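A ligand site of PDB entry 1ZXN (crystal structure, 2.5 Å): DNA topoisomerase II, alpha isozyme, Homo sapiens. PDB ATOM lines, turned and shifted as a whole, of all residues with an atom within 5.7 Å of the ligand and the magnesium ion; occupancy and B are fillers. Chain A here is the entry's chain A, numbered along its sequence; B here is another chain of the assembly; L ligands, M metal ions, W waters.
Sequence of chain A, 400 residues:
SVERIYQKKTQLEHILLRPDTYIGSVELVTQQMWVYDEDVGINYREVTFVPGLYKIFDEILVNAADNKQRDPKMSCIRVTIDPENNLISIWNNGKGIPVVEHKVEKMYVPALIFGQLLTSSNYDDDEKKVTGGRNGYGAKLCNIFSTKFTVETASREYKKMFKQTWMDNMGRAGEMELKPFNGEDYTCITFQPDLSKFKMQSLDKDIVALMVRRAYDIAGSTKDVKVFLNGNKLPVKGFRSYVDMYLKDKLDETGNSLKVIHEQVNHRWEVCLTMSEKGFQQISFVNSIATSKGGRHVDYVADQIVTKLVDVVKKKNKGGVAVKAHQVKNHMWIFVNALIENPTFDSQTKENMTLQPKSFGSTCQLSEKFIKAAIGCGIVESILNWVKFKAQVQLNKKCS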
ATOM      1  N   GLU A  59      30.087  -4.339  -0.453  1.00  0.00           N
ATOM      2  CA  GLU A  59      29.054  -5.085  -1.140  1.00  0.00           C
ATOM      3  C   GLU A  59      28.528  -4.382  -2.399  1.00  0.00           C
ATOM      4  O   GLU A  59      28.356  -5.013  -3.449  1.00  0.00           O
ATOM      5  CB  GLU A  59      27.903  -5.401  -0.179  1.00  0.00           C
ATOM      6  CG  GLU A  59      28.312  -6.263   1.012  1.00  0.00           C
ATOM      7  CD  GLU A  59      28.925  -7.599   0.605  1.00  0.00           C
ATOM      8  OE1 GLU A  59      29.773  -8.134   1.361  1.00  0.00           O
ATOM      9  OE2 GLU A  59      28.566  -8.130  -0.478  1.00  0.00           O
ATOM     10  N   VAL A  62      31.533  -4.152  -5.134  1.00  0.00           N
ATOM     11  CA  VAL A  62      31.738  -5.390  -5.866  1.00  0.00           C
ATOM     12  C   VAL A  62      30.578  -5.694  -6.828  1.00  0.00           C
ATOM     13  O   VAL A  62      30.800  -6.204  -7.918  1.00  0.00           O
ATOM     14  CB  VAL A  62      31.956  -6.553  -4.916  1.00  0.00           C
ATOM     15  CG1 VAL A  62      32.107  -7.835  -5.701  1.00  0.00           C
ATOM     16  CG2 VAL A  62      33.207  -6.299  -4.076  1.00  0.00           C
ATOM     17  N   ASN A  63      29.353  -5.376  -6.425  1.00  0.00           N
ATOM     18  CA  ASN A  63      28.216  -5.626  -7.297  1.00  0.00           C
ATOM     19  C   ASN A  63      28.481  -4.838  -8.571  1.00  0.00           C
ATOM     20  O   ASN A  63      28.212  -5.325  -9.657  1.00  0.00           O
ATOM     21  CB  ASN A  63      26.893  -5.162  -6.668  1.00  0.00           C
ATOM     22  CG  ASN A  63      26.370  -6.132  -5.598  1.00  0.00           C
ATOM     23  OD1 ASN A  63      26.742  -7.319  -5.569  1.00  0.00           O
ATOM     24  ND2 ASN A  63      25.479  -5.641  -4.745  1.00  0.00           N
ATOM     25  N   ALA A  64      29.006  -3.622  -8.428  1.00  0.00           N
ATOM     26  CA  ALA A  64      29.307  -2.758  -9.574  1.00  0.00           C
ATOM     27  C   ALA A  64      30.307  -3.459 -10.466  1.00  0.00           C
ATOM     28  O   ALA A  64      30.116  -3.547 -11.681  1.00  0.00           O
ATOM     29  CB  ALA A  64      29.888  -1.434  -9.098  1.00  0.00           C
ATOM     30  N   ASP A  66      31.012  -6.678 -10.471  1.00  0.00           N
ATOM     31  CA  ASP A  66      30.372  -7.877 -10.975  1.00  0.00           C
ATOM     32  C   ASP A  66      29.669  -7.657 -12.313  1.00  0.00           C
ATOM     33  O   ASP A  66      29.663  -8.538 -13.172  1.00  0.00           O
ATOM     34  CB  ASP A  66      29.372  -8.445  -9.964  1.00  0.00           C
ATOM     35  CG  ASP A  66      30.036  -9.198  -8.843  1.00  0.00           C
ATOM     36  OD1 ASP A  66      31.178  -9.659  -9.055  1.00  0.00           O
ATOM     37  OD2 ASP A  66      29.424  -9.350  -7.752  1.00  0.00           O
ATOM     38  N   ASN A  67      29.077  -6.476 -12.492  1.00  0.00           N
ATOM     39  CA  ASN A  67      28.362  -6.209 -13.729  1.00  0.00           C
ATOM     40  C   ASN A  67      29.253  -6.247 -14.967  1.00  0.00           C
ATOM     41  O   ASN A  67      28.752  -6.276 -16.095  1.00  0.00           O
ATOM     42  CB  ASN A  67      27.659  -4.862 -13.662  1.00  0.00           C
ATOM     43  CG  ASN A  67      26.517  -4.765 -14.652  1.00  0.00           C
ATOM     44  OD1 ASN A  67      25.579  -5.575 -14.594  1.00  0.00           O
ATOM     45  ND2 ASN A  67      26.588  -3.796 -15.568  1.00  0.00           N
ATOM     46  N   ARG A  70      28.829  -9.725 -16.388  1.00  0.00           N
ATOM     47  CA  ARG A  70      27.509  -9.816 -16.983  1.00  0.00           C
ATOM     48  C   ARG A  70      27.440  -9.076 -18.322  1.00  0.00           C
ATOM     49  O   ARG A  70      26.637  -9.404 -19.187  1.00  0.00           O
ATOM     50  CB  ARG A  70      26.467  -9.224 -16.032  1.00  0.00           C
ATOM     51  CG  ARG A  70      25.051  -9.210 -16.573  1.00  0.00           C
ATOM     52  CD  ARG A  70      24.182  -8.206 -15.856  1.00  0.00           C
ATOM     53  NE  ARG A  70      22.861  -8.080 -16.462  1.00  0.00           N
ATOM     54  CZ  ARG A  70      22.099  -6.990 -16.378  1.00  0.00           C
ATOM     55  NH1 ARG A  70      22.549  -5.929 -15.707  1.00  0.00           N
ATOM     56  NH2 ARG A  70      20.906  -6.944 -16.951  1.00  0.00           N
ATOM     57  N   ASN A  92      27.511   2.670 -12.249  1.00  0.00           N
ATOM     58  CA  ASN A  92      28.192   1.862 -13.247  1.00  0.00           C
ATOM     59  C   ASN A  92      27.441   1.909 -14.567  1.00  0.00           C
ATOM     60  O   ASN A  92      26.231   2.131 -14.593  1.00  0.00           O
ATOM     61  CB  ASN A  92      28.355   0.390 -12.795  1.00  0.00           C
ATOM     62  CG  ASN A  92      27.015  -0.291 -12.481  1.00  0.00           C
ATOM     63  OD1 ASN A  92      26.439  -0.111 -11.402  1.00  0.00           O
ATOM     64  ND2 ASN A  92      26.517  -1.071 -13.444  1.00  0.00           N
ATOM     65  N   LYS A  95      24.867  -2.971 -19.242  1.00  0.00           N
ATOM     66  CA  LYS A  95      23.450  -3.334 -19.252  1.00  0.00           C
ATOM     67  C   LYS A  95      22.847  -3.067 -17.890  1.00  0.00           C
ATOM     68  O   LYS A  95      23.382  -3.497 -16.869  1.00  0.00           O
ATOM     69  CB  LYS A  95      23.274  -4.814 -19.638  1.00  0.00           C
ATOM     70  N   GLY A  96      21.745  -2.328 -17.876  1.00  0.00           N
ATOM     71  CA  GLY A  96      21.086  -2.021 -16.630  1.00  0.00           C
ATOM     72  C   GLY A  96      20.341  -3.246 -16.117  1.00  0.00           C
ATOM     73  O   GLY A  96      20.531  -4.371 -16.634  1.00  0.00           O
ATOM     74  N   ILE A  97      19.497  -3.046 -15.116  1.00  0.00           N
ATOM     75  CA  ILE A  97      18.738  -4.160 -14.574  1.00  0.00           C
ATOM     76  C   ILE A  97      17.376  -4.177 -15.245  1.00  0.00           C
ATOM     77  O   ILE A  97      16.716  -3.145 -15.364  1.00  0.00           O
ATOM     78  CB  ILE A  97      18.582  -4.018 -13.036  1.00  0.00           C
ATOM     79  CG1 ILE A  97      19.968  -3.968 -12.398  1.00  0.00           C
ATOM     80  CG2 ILE A  97      17.769  -5.189 -12.475  1.00  0.00           C
ATOM     81  CD1 ILE A  97      19.953  -3.741 -10.909  1.00  0.00           C
ATOM     82  N   ILE A 113      15.349  -7.743  -6.216  1.00  0.00           N
ATOM     83  CA  ILE A 113      16.735  -8.020  -5.801  1.00  0.00           C
ATOM     84  C   ILE A 113      17.446  -7.008  -4.893  1.00  0.00           C
ATOM     85  O   ILE A 113      18.595  -7.220  -4.496  1.00  0.00           O
ATOM     86  CB  ILE A 113      17.617  -8.295  -7.042  1.00  0.00           C
ATOM     87  CG1 ILE A 113      17.785  -7.038  -7.875  1.00  0.00           C
ATOM     88  CG2 ILE A 113      16.967  -9.384  -7.906  1.00  0.00           C
ATOM     89  CD1 ILE A 113      18.449  -7.291  -9.186  1.00  0.00           C
ATOM     90  N   PHE A 114      16.788  -5.910  -4.545  1.00  0.00           N
ATOM     91  CA  PHE A 114      17.398  -4.916  -3.656  1.00  0.00           C
ATOM     92  C   PHE A 114      16.568  -4.737  -2.385  1.00  0.00           C
ATOM     93  O   PHE A 114      17.047  -4.153  -1.407  1.00  0.00           O
ATOM     94  CB  PHE A 114      17.543  -3.566  -4.362  1.00  0.00           C
ATOM     95  CG  PHE A 114      18.789  -3.440  -5.189  1.00  0.00           C
ATOM     96  CD1 PHE A 114      20.015  -3.162  -4.585  1.00  0.00           C
ATOM     97  CD2 PHE A 114      18.744  -3.593  -6.580  1.00  0.00           C
ATOM     98  CE1 PHE A 114      21.195  -3.033  -5.364  1.00  0.00           C
ATOM     99  CE2 PHE A 114      19.893  -3.468  -7.362  1.00  0.00           C
ATOM    100  CZ  PHE A 114      21.128  -3.186  -6.748  1.00  0.00           C
ATOM    101  N   THR A 119      17.741 -12.939  -2.621  1.00  0.00           N
ATOM    102  CA  THR A 119      17.455 -12.758  -4.040  1.00  0.00           C
ATOM    103  C   THR A 119      18.777 -12.588  -4.747  1.00  0.00           C
ATOM    104  O   THR A 119      19.627 -11.829  -4.293  1.00  0.00           O
ATOM    105  CB  THR A 119      16.554 -11.525  -4.290  1.00  0.00           C
ATOM    106  OG1 THR A 119      17.062 -10.405  -3.576  1.00  0.00           O
ATOM    107  CG2 THR A 119      15.103 -11.824  -3.852  1.00  0.00           C
ATOM    108  N   SER A 120      18.950 -13.285  -5.859  1.00  0.00           N
ATOM    109  CA  SER A 120      20.224 -13.235  -6.562  1.00  0.00           C
ATOM    110  C   SER A 120      20.166 -13.840  -7.962  1.00  0.00           C
ATOM    111  O   SER A 120      19.244 -14.586  -8.301  1.00  0.00           O
ATOM    112  CB  SER A 120      21.268 -13.996  -5.715  1.00  0.00           C
ATOM    113  OG  SER A 120      22.519 -14.177  -6.365  1.00  0.00           O
ATOM    114  N   SER A 121      21.148 -13.511  -8.800  1.00  0.00           N
ATOM    115  CA  SER A 121      21.220 -14.049 -10.149  1.00  0.00           C
ATOM    116  C   SER A 121      22.439 -14.955 -10.206  1.00  0.00           C
ATOM    117  O   SER A 121      22.867 -15.369 -11.278  1.00  0.00           O
ATOM    118  CB  SER A 121      21.363 -12.948 -11.186  1.00  0.00           C
ATOM    119  OG  SER A 121      22.553 -12.219 -10.985  1.00  0.00           O
ATOM    120  N   ASN A 122      23.010 -15.257  -9.034  1.00  0.00           N
ATOM    121  CA  ASN A 122      24.168 -16.123  -8.969  1.00  0.00           C
ATOM    122  C   ASN A 122      23.839 -17.403  -8.210  1.00  0.00           C
ATOM    123  O   ASN A 122      24.730 -18.036  -7.651  1.00  0.00           O
ATOM    124  CB  ASN A 122      25.338 -15.425  -8.270  1.00  0.00           C
ATOM    125  CG  ASN A 122      25.694 -14.089  -8.914  1.00  0.00           C
ATOM    126  OD1 ASN A 122      25.904 -14.011 -10.139  1.00  0.00           O
ATOM    127  ND2 ASN A 122      25.776 -13.033  -8.094  1.00  0.00           N
ATOM    128  N   GLY A 132      31.704 -11.904  -7.763  1.00  0.00           N
ATOM    129  CA  GLY A 132      31.886 -11.964  -6.327  1.00  0.00           C
ATOM    130  C   GLY A 132      30.534 -12.305  -5.738  1.00  0.00           C
ATOM    131  O   GLY A 132      30.443 -12.872  -4.645  1.00  0.00           O
ATOM    132  N   GLY A 133      29.484 -11.936  -6.485  1.00  0.00           N
ATOM    133  CA  GLY A 133      28.114 -12.209  -6.063  1.00  0.00           C
ATOM    134  C   GLY A 133      27.912 -13.697  -5.882  1.00  0.00           C
ATOM    135  O   GLY A 133      28.395 -14.488  -6.691  1.00  0.00           O
ATOM    136  N   ARG A 134      27.179 -14.082  -4.843  1.00  0.00           N
ATOM    137  CA  ARG A 134      26.983 -15.500  -4.612  1.00  0.00           C
ATOM    138  C   ARG A 134      25.861 -15.879  -3.638  1.00  0.00           C
ATOM    139  O   ARG A 134      25.047 -16.742  -3.933  1.00  0.00           O
ATOM    140  CB  ARG A 134      28.293 -16.077  -4.103  1.00  0.00           C
ATOM    141  CG  ARG A 134      28.337 -17.554  -4.085  1.00  0.00           C
ATOM    142  CD  ARG A 134      29.275 -18.009  -3.020  1.00  0.00           C
ATOM    143  NE  ARG A 134      29.307 -19.453  -2.940  1.00  0.00           N
ATOM    144  CZ  ARG A 134      29.677 -20.126  -1.858  1.00  0.00           C
ATOM    145  NH1 ARG A 134      30.058 -19.463  -0.755  1.00  0.00           N
ATOM    146  NH2 ARG A 134      29.649 -21.446  -1.882  1.00  0.00           N
ATOM    147  N   ASN A 135      25.825 -15.230  -2.477  1.00  0.00           N
ATOM    148  CA  ASN A 135      24.820 -15.537  -1.471  1.00  0.00           C
ATOM    149  C   ASN A 135      23.497 -14.803  -1.570  1.00  0.00           C
ATOM    150  O   ASN A 135      22.522 -15.231  -0.985  1.00  0.00           O
ATOM    151  CB  ASN A 135      25.406 -15.318  -0.076  1.00  0.00           C
ATOM    152  CG  ASN A 135      26.400 -16.391   0.325  1.00  0.00           C
ATOM    153  OD1 ASN A 135      27.444 -16.541  -0.286  1.00  0.00           O
ATOM    154  ND2 ASN A 135      26.057 -17.147   1.371  1.00  0.00           N
ATOM    155  N   GLY A 136      23.460 -13.701  -2.303  1.00  0.00           N
ATOM    156  CA  GLY A 136      22.218 -12.956  -2.420  1.00  0.00           C
ATOM    157  C   GLY A 136      21.829 -12.100  -1.214  1.00  0.00           C
ATOM    158  O   GLY A 136      20.663 -11.707  -1.095  1.00  0.00           O
ATOM    159  N   TYR A 137      22.777 -11.817  -0.327  1.00  0.00           N
ATOM    160  CA  TYR A 137      22.509 -10.980   0.853  1.00  0.00           C
ATOM    161  C   TYR A 137      22.958  -9.519   0.675  1.00  0.00           C
ATOM    162  O   TYR A 137      22.211  -8.598   0.998  1.00  0.00           O
ATOM    163  CB  TYR A 137      23.228 -11.536   2.090  1.00  0.00           C
ATOM    164  CG  TYR A 137      22.429 -12.510   2.948  1.00  0.00           C
ATOM    165  CD1 TYR A 137      22.748 -13.866   2.979  1.00  0.00           C
ATOM    166  CD2 TYR A 137      21.392 -12.062   3.780  1.00  0.00           C
ATOM    167  CE1 TYR A 137      22.073 -14.751   3.807  1.00  0.00           C
ATOM    168  CE2 TYR A 137      20.699 -12.944   4.603  1.00  0.00           C
ATOM    169  CZ  TYR A 137      21.047 -14.291   4.607  1.00  0.00           C
ATOM    170  OH  TYR A 137      20.378 -15.193   5.411  1.00  0.00           O
ATOM    171  N   GLY A 138      24.193  -9.369   0.193  1.00  0.00           N
ATOM    172  CA  GLY A 138      24.845  -8.087  -0.041  1.00  0.00           C
ATOM    173  C   GLY A 138      24.085  -6.773  -0.123  1.00  0.00           C
ATOM    174  O   GLY A 138      24.074  -5.986   0.828  1.00  0.00           O
ATOM    175  N   ALA A 139      23.482  -6.508  -1.274  1.00  0.00           N
ATOM    176  CA  ALA A 139      22.740  -5.265  -1.452  1.00  0.00           C
ATOM    177  C   ALA A 139      21.695  -5.057  -0.368  1.00  0.00           C
ATOM    178  O   ALA A 139      21.409  -3.916   0.017  1.00  0.00           O
ATOM    179  CB  ALA A 139      22.096  -5.258  -2.835  1.00  0.00           C
ATOM    180  N   LYS A 140      21.110  -6.147   0.126  1.00  0.00           N
ATOM    181  CA  LYS A 140      20.097  -6.027   1.167  1.00  0.00           C
ATOM    182  C   LYS A 140      20.710  -5.642   2.506  1.00  0.00           C
ATOM    183  O   LYS A 140      20.136  -4.856   3.264  1.00  0.00           O
ATOM    184  CB  LYS A 140      19.288  -7.327   1.283  1.00  0.00           C
ATOM    185  CG  LYS A 140      18.110  -7.429   0.295  1.00  0.00           C
ATOM    186  CD  LYS A 140      18.558  -7.652  -1.166  1.00  0.00           C
ATOM    187  CE  LYS A 140      19.301  -8.972  -1.322  1.00  0.00           C
ATOM    188  NZ  LYS A 140      19.613  -9.329  -2.734  1.00  0.00           N
ATOM    189  N   THR A 187      23.276   2.154 -13.619  1.00  0.00           N
ATOM    190  CA  THR A 187      22.698   1.779 -12.344  1.00  0.00           C
ATOM    191  C   THR A 187      23.445   2.580 -11.287  1.00  0.00           C
ATOM    192  O   THR A 187      24.670   2.664 -11.320  1.00  0.00           O
ATOM    193  CB  THR A 187      22.863   0.266 -12.064  1.00  0.00           C
ATOM    194  OG1 THR A 187      21.933  -0.470 -12.852  1.00  0.00           O
ATOM    195  CG2 THR A 187      22.615  -0.047 -10.596  1.00  0.00           C
ATOM    196  N   TYR B   6      16.943 -14.167 -12.261  1.00  0.00           N
ATOM    197  CA  TYR B   6      16.816 -13.594 -10.923  1.00  0.00           C
ATOM    198  C   TYR B   6      15.941 -14.485 -10.090  1.00  0.00           C
ATOM    199  O   TYR B   6      14.734 -14.603 -10.356  1.00  0.00           O
ATOM    200  CB  TYR B   6      16.217 -12.204 -11.019  1.00  0.00           C
ATOM    201  CG  TYR B   6      17.053 -11.268 -11.842  1.00  0.00           C
ATOM    202  CD1 TYR B   6      18.151 -10.613 -11.277  1.00  0.00           C
ATOM    203  CD2 TYR B   6      16.781 -11.052 -13.184  1.00  0.00           C
ATOM    204  CE1 TYR B   6      18.936  -9.765 -12.032  1.00  0.00           C
ATOM    205  CE2 TYR B   6      17.557 -10.223 -13.952  1.00  0.00           C
ATOM    206  CZ  TYR B   6      18.641  -9.569 -13.377  1.00  0.00           C
ATOM    207  OH  TYR B   6      19.387  -8.696 -14.132  1.00  0.00           O
HETATM  208  P1  LIG L   1      24.739 -11.373  -4.901  1.00  0.00           P
HETATM  209  O1  LIG L   1      24.115 -11.949  -6.102  1.00  0.00           O
HETATM  210  O2  LIG L   1      25.299 -12.372  -3.970  1.00  0.00           O
HETATM  211  O3  LIG L   1      25.801 -10.307  -5.388  1.00  0.00           O
HETATM  212  P2  LIG L   1      23.368  -9.071  -3.853  1.00  0.00           P
HETATM  213  O4  LIG L   1      22.614  -8.863  -2.577  1.00  0.00           O
HETATM  214  O5  LIG L   1      24.692  -8.363  -3.914  1.00  0.00           O
HETATM  215  O6  LIG L   1      23.568 -10.617  -4.120  1.00  0.00           O
HETATM  216  O7  LIG L   1      22.318  -8.700  -4.929  1.00  0.00           O
HETATM  217  C1  LIG L   1      22.745  -8.820  -6.268  1.00  0.00           C
HETATM  218  C2  LIG L   1      21.653  -9.066  -7.260  1.00  0.00           C
HETATM  219  O8  LIG L   1      21.321  -7.763  -7.782  1.00  0.00           O
HETATM  220  C3  LIG L   1      22.073  -9.917  -8.463  1.00  0.00           C
HETATM  221  O9  LIG L   1      20.936 -10.744  -8.858  1.00  0.00           O
HETATM  222  C4  LIG L   1      22.531  -8.872  -9.489  1.00  0.00           C
HETATM  223  O10 LIG L   1      22.175  -9.272 -10.819  1.00  0.00           O
HETATM  224  C5  LIG L   1      21.827  -7.561  -9.106  1.00  0.00           C
HETATM  225  N1  LIG L   1      22.790  -6.359  -9.108  1.00  0.00           N
HETATM  226  C6  LIG L   1      23.431  -5.795  -8.046  1.00  0.00           C
HETATM  227  N2  LIG L   1      24.199  -4.753  -8.357  1.00  0.00           N
HETATM  228  C7  LIG L   1      24.058  -4.636  -9.690  1.00  0.00           C
HETATM  229  C8  LIG L   1      24.636  -3.701 -10.674  1.00  0.00           C
HETATM  230  N3  LIG L   1      25.452  -2.738 -10.415  1.00  0.00           N
HETATM  231  N4  LIG L   1      24.225  -3.920 -11.985  1.00  0.00           N
HETATM  232  C9  LIG L   1      23.331  -4.956 -12.369  1.00  0.00           C
HETATM  233  N5  LIG L   1      22.802  -5.811 -11.485  1.00  0.00           N
HETATM  234  C10 LIG L   1      23.181  -5.630 -10.189  1.00  0.00           C
HETATM  235 MG    MG M   1      26.629  -8.790  -4.215  1.00  0.00          MG
HETATM  236  O   HOH W   1      28.476  -9.357  -4.857  1.00  0.00           O
HETATM  237  O   HOH W   2      27.608  -7.613  -2.587  1.00  0.00           O
HETATM  238  O   HOH W   3      26.035  -7.030  -9.738  1.00  0.00           O
HETATM  239  O   HOH W   4      23.845  -2.034 -14.141  1.00  0.00           O
HETATM  240  O   HOH W   5      27.119 -10.909  -2.332  1.00  0.00           O
HETATM  241  O   HOH W   6      24.187  -3.037  -5.943  1.00  0.00           O
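Of the 28 residues printed, 1 comes within 4 Å of the magnesium ion.
The nearest printed residue that does not touch the magnesium ion is Gly 133 (4.2 Å).
ND2 of Asn 63 sits close to O of Glu 59.
The backbone carbonyl oxygen of Gly 133 sits close to the side-chain amide nitrogen of Asn 122 (3.3 Å).
The side-chain amide nitrogen of Asn 92 sits close to the side-chain amide nitrogen of Asn 67 (3.5 Å).
The backbone NH (N) of Asn 92 is in hydrogen-bond range of the backbone carbonyl oxygen (O) of Thr 187.
The side-chain amino group (NZ) of Lys 140 is in hydrogen-bond range of the backbone carbonyl oxygen (O) of Ile 113 (2.9 Å).
The backbone NH of Gly 133 is in hydrogen-bond range of the side-chain carboxylate of Asp 66 (2.9 Å).
OD1 of Asn 67 sits close to NH1 of Arg 70 (3.2 Å).
The guanidinium group (NH1) of Arg 70 sits at hydrogen-bond distance from the backbone carbonyl oxygen (O) of Lys 95, at 2.8 Å.
O2 of the ligand is in hydrogen-bond range of N of Arg 134, at 2.7 Å.
The side-chain hydroxyl of Ser 120 lies within hydrogen-bond range of an oxygen (O1) of the ligand, at 2.8 Å.
The backbone NH (N) of Ser 121 sits at hydrogen-bond distance from an oxygen (O9) of the ligand, 2.8 Å away.
OG of Ser 121 sits at hydrogen-bond distance from O10 of the ligand (3.0 Å).
ND2 of Asn 122 lies within hydrogen-bond range of O1 of the ligand (2.8 Å).
An oxygen (O2) of the ligand lies within hydrogen-bond range of the backbone NH (N) of Gly 136 (2.8 Å).
An oxygen (O4) of the ligand lies within hydrogen-bond range of the backbone NH (N) of Ala 139, 2.8 Å away.
The side-chain amide oxygen (OD1) of Asn 92 is in hydrogen-bond range of a nitrogen (N3) of the ligand (3.0 Å).
The side-chain amino group (NZ) of Lys 140 lies within salt-bridge range of an oxygen (O4) of the ligand, at 3.0 Å.
N4 of the ligand sits close to OD1 of Asn 67, at 3.4 Å.
The backbone NH (N) of Gly 138 sits at hydrogen-bond distance from an oxygen (O4) of the ligand (3.2 Å).
N of Asn 135 sits at hydrogen-bond distance from O2 of the ligand (3.3 Å).
OD1 of Asn 63 is bound to the magnesium ion (2.0 Å).
The magnesium ion is bound by an oxygen (O5) of the ligand (2.0 Å).
The magnesium ion is bound by water W1, at 2.0 Å.
The magnesium ion is bound by O3 of the ligand (2.1 Å).
The magnesium ion is bound by water W2.
Water W1 lies within hydrogen-bond range of OD2 of Asp 66 (3.0 Å) and N of Gly 133 (3.2 Å).
Water W4 lies within hydrogen-bond range of the side-chain hydroxyl (OG1) of Thr 187 (2.8 Å), a nitrogen (N4) of the ligand (2.9 Å), the side-chain amide nitrogen (ND2) of Asn 92 (2.9 Å) and the backbone carbonyl oxygen (O) of Lys 95 (3.1 Å).
Water W6 bridges N2 of the ligand and ND2 of Asn 63.
Water W3 lies within hydrogen-bond range of the backbone carbonyl oxygen of Asn 63 (2.8 Å) and a nitrogen (N2) of the ligand (3.2 Å).
Ala 64 touches the ligand.
Arg 70 touches the ligand (NH1 to C9, 3.6 Å).
CG1 of Ile 97 touches N5 of the ligand, at 3.5 Å.
Ile 113 touches the ligand.
Phe 114 touches the ligand.
Gly 133 touches the ligand (CA to O3, 3.1 Å).
Tyr 137 touches the ligand (C to O4, 3.3 Å).
Thr 187 touches the ligand.
CE1 of Tyr 6 of chain B touches O10 of the ligand (3.5 Å).
Hydrophobic or aromatic side chains that line the ligand: Ile 97, Ile 113, Phe 114, Ala 139 and Tyr 6 of chain B.
Within 4 Å of the ligand: Asn 63, Ala 64, Asn 67, Arg 70, Asn 92, Ile 97, Ile 113, Phe 114, Ser 120, Ser 121, Asn 122, Gly 133, Arg 134, Asn 135, Gly 136, Tyr 137, Gly 138, Ala 139, Lys 140, Thr 187 and Tyr 6 of chain B.
The nearest printed residue that does not touch the ligand is Thr 119 (4.1 Å).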
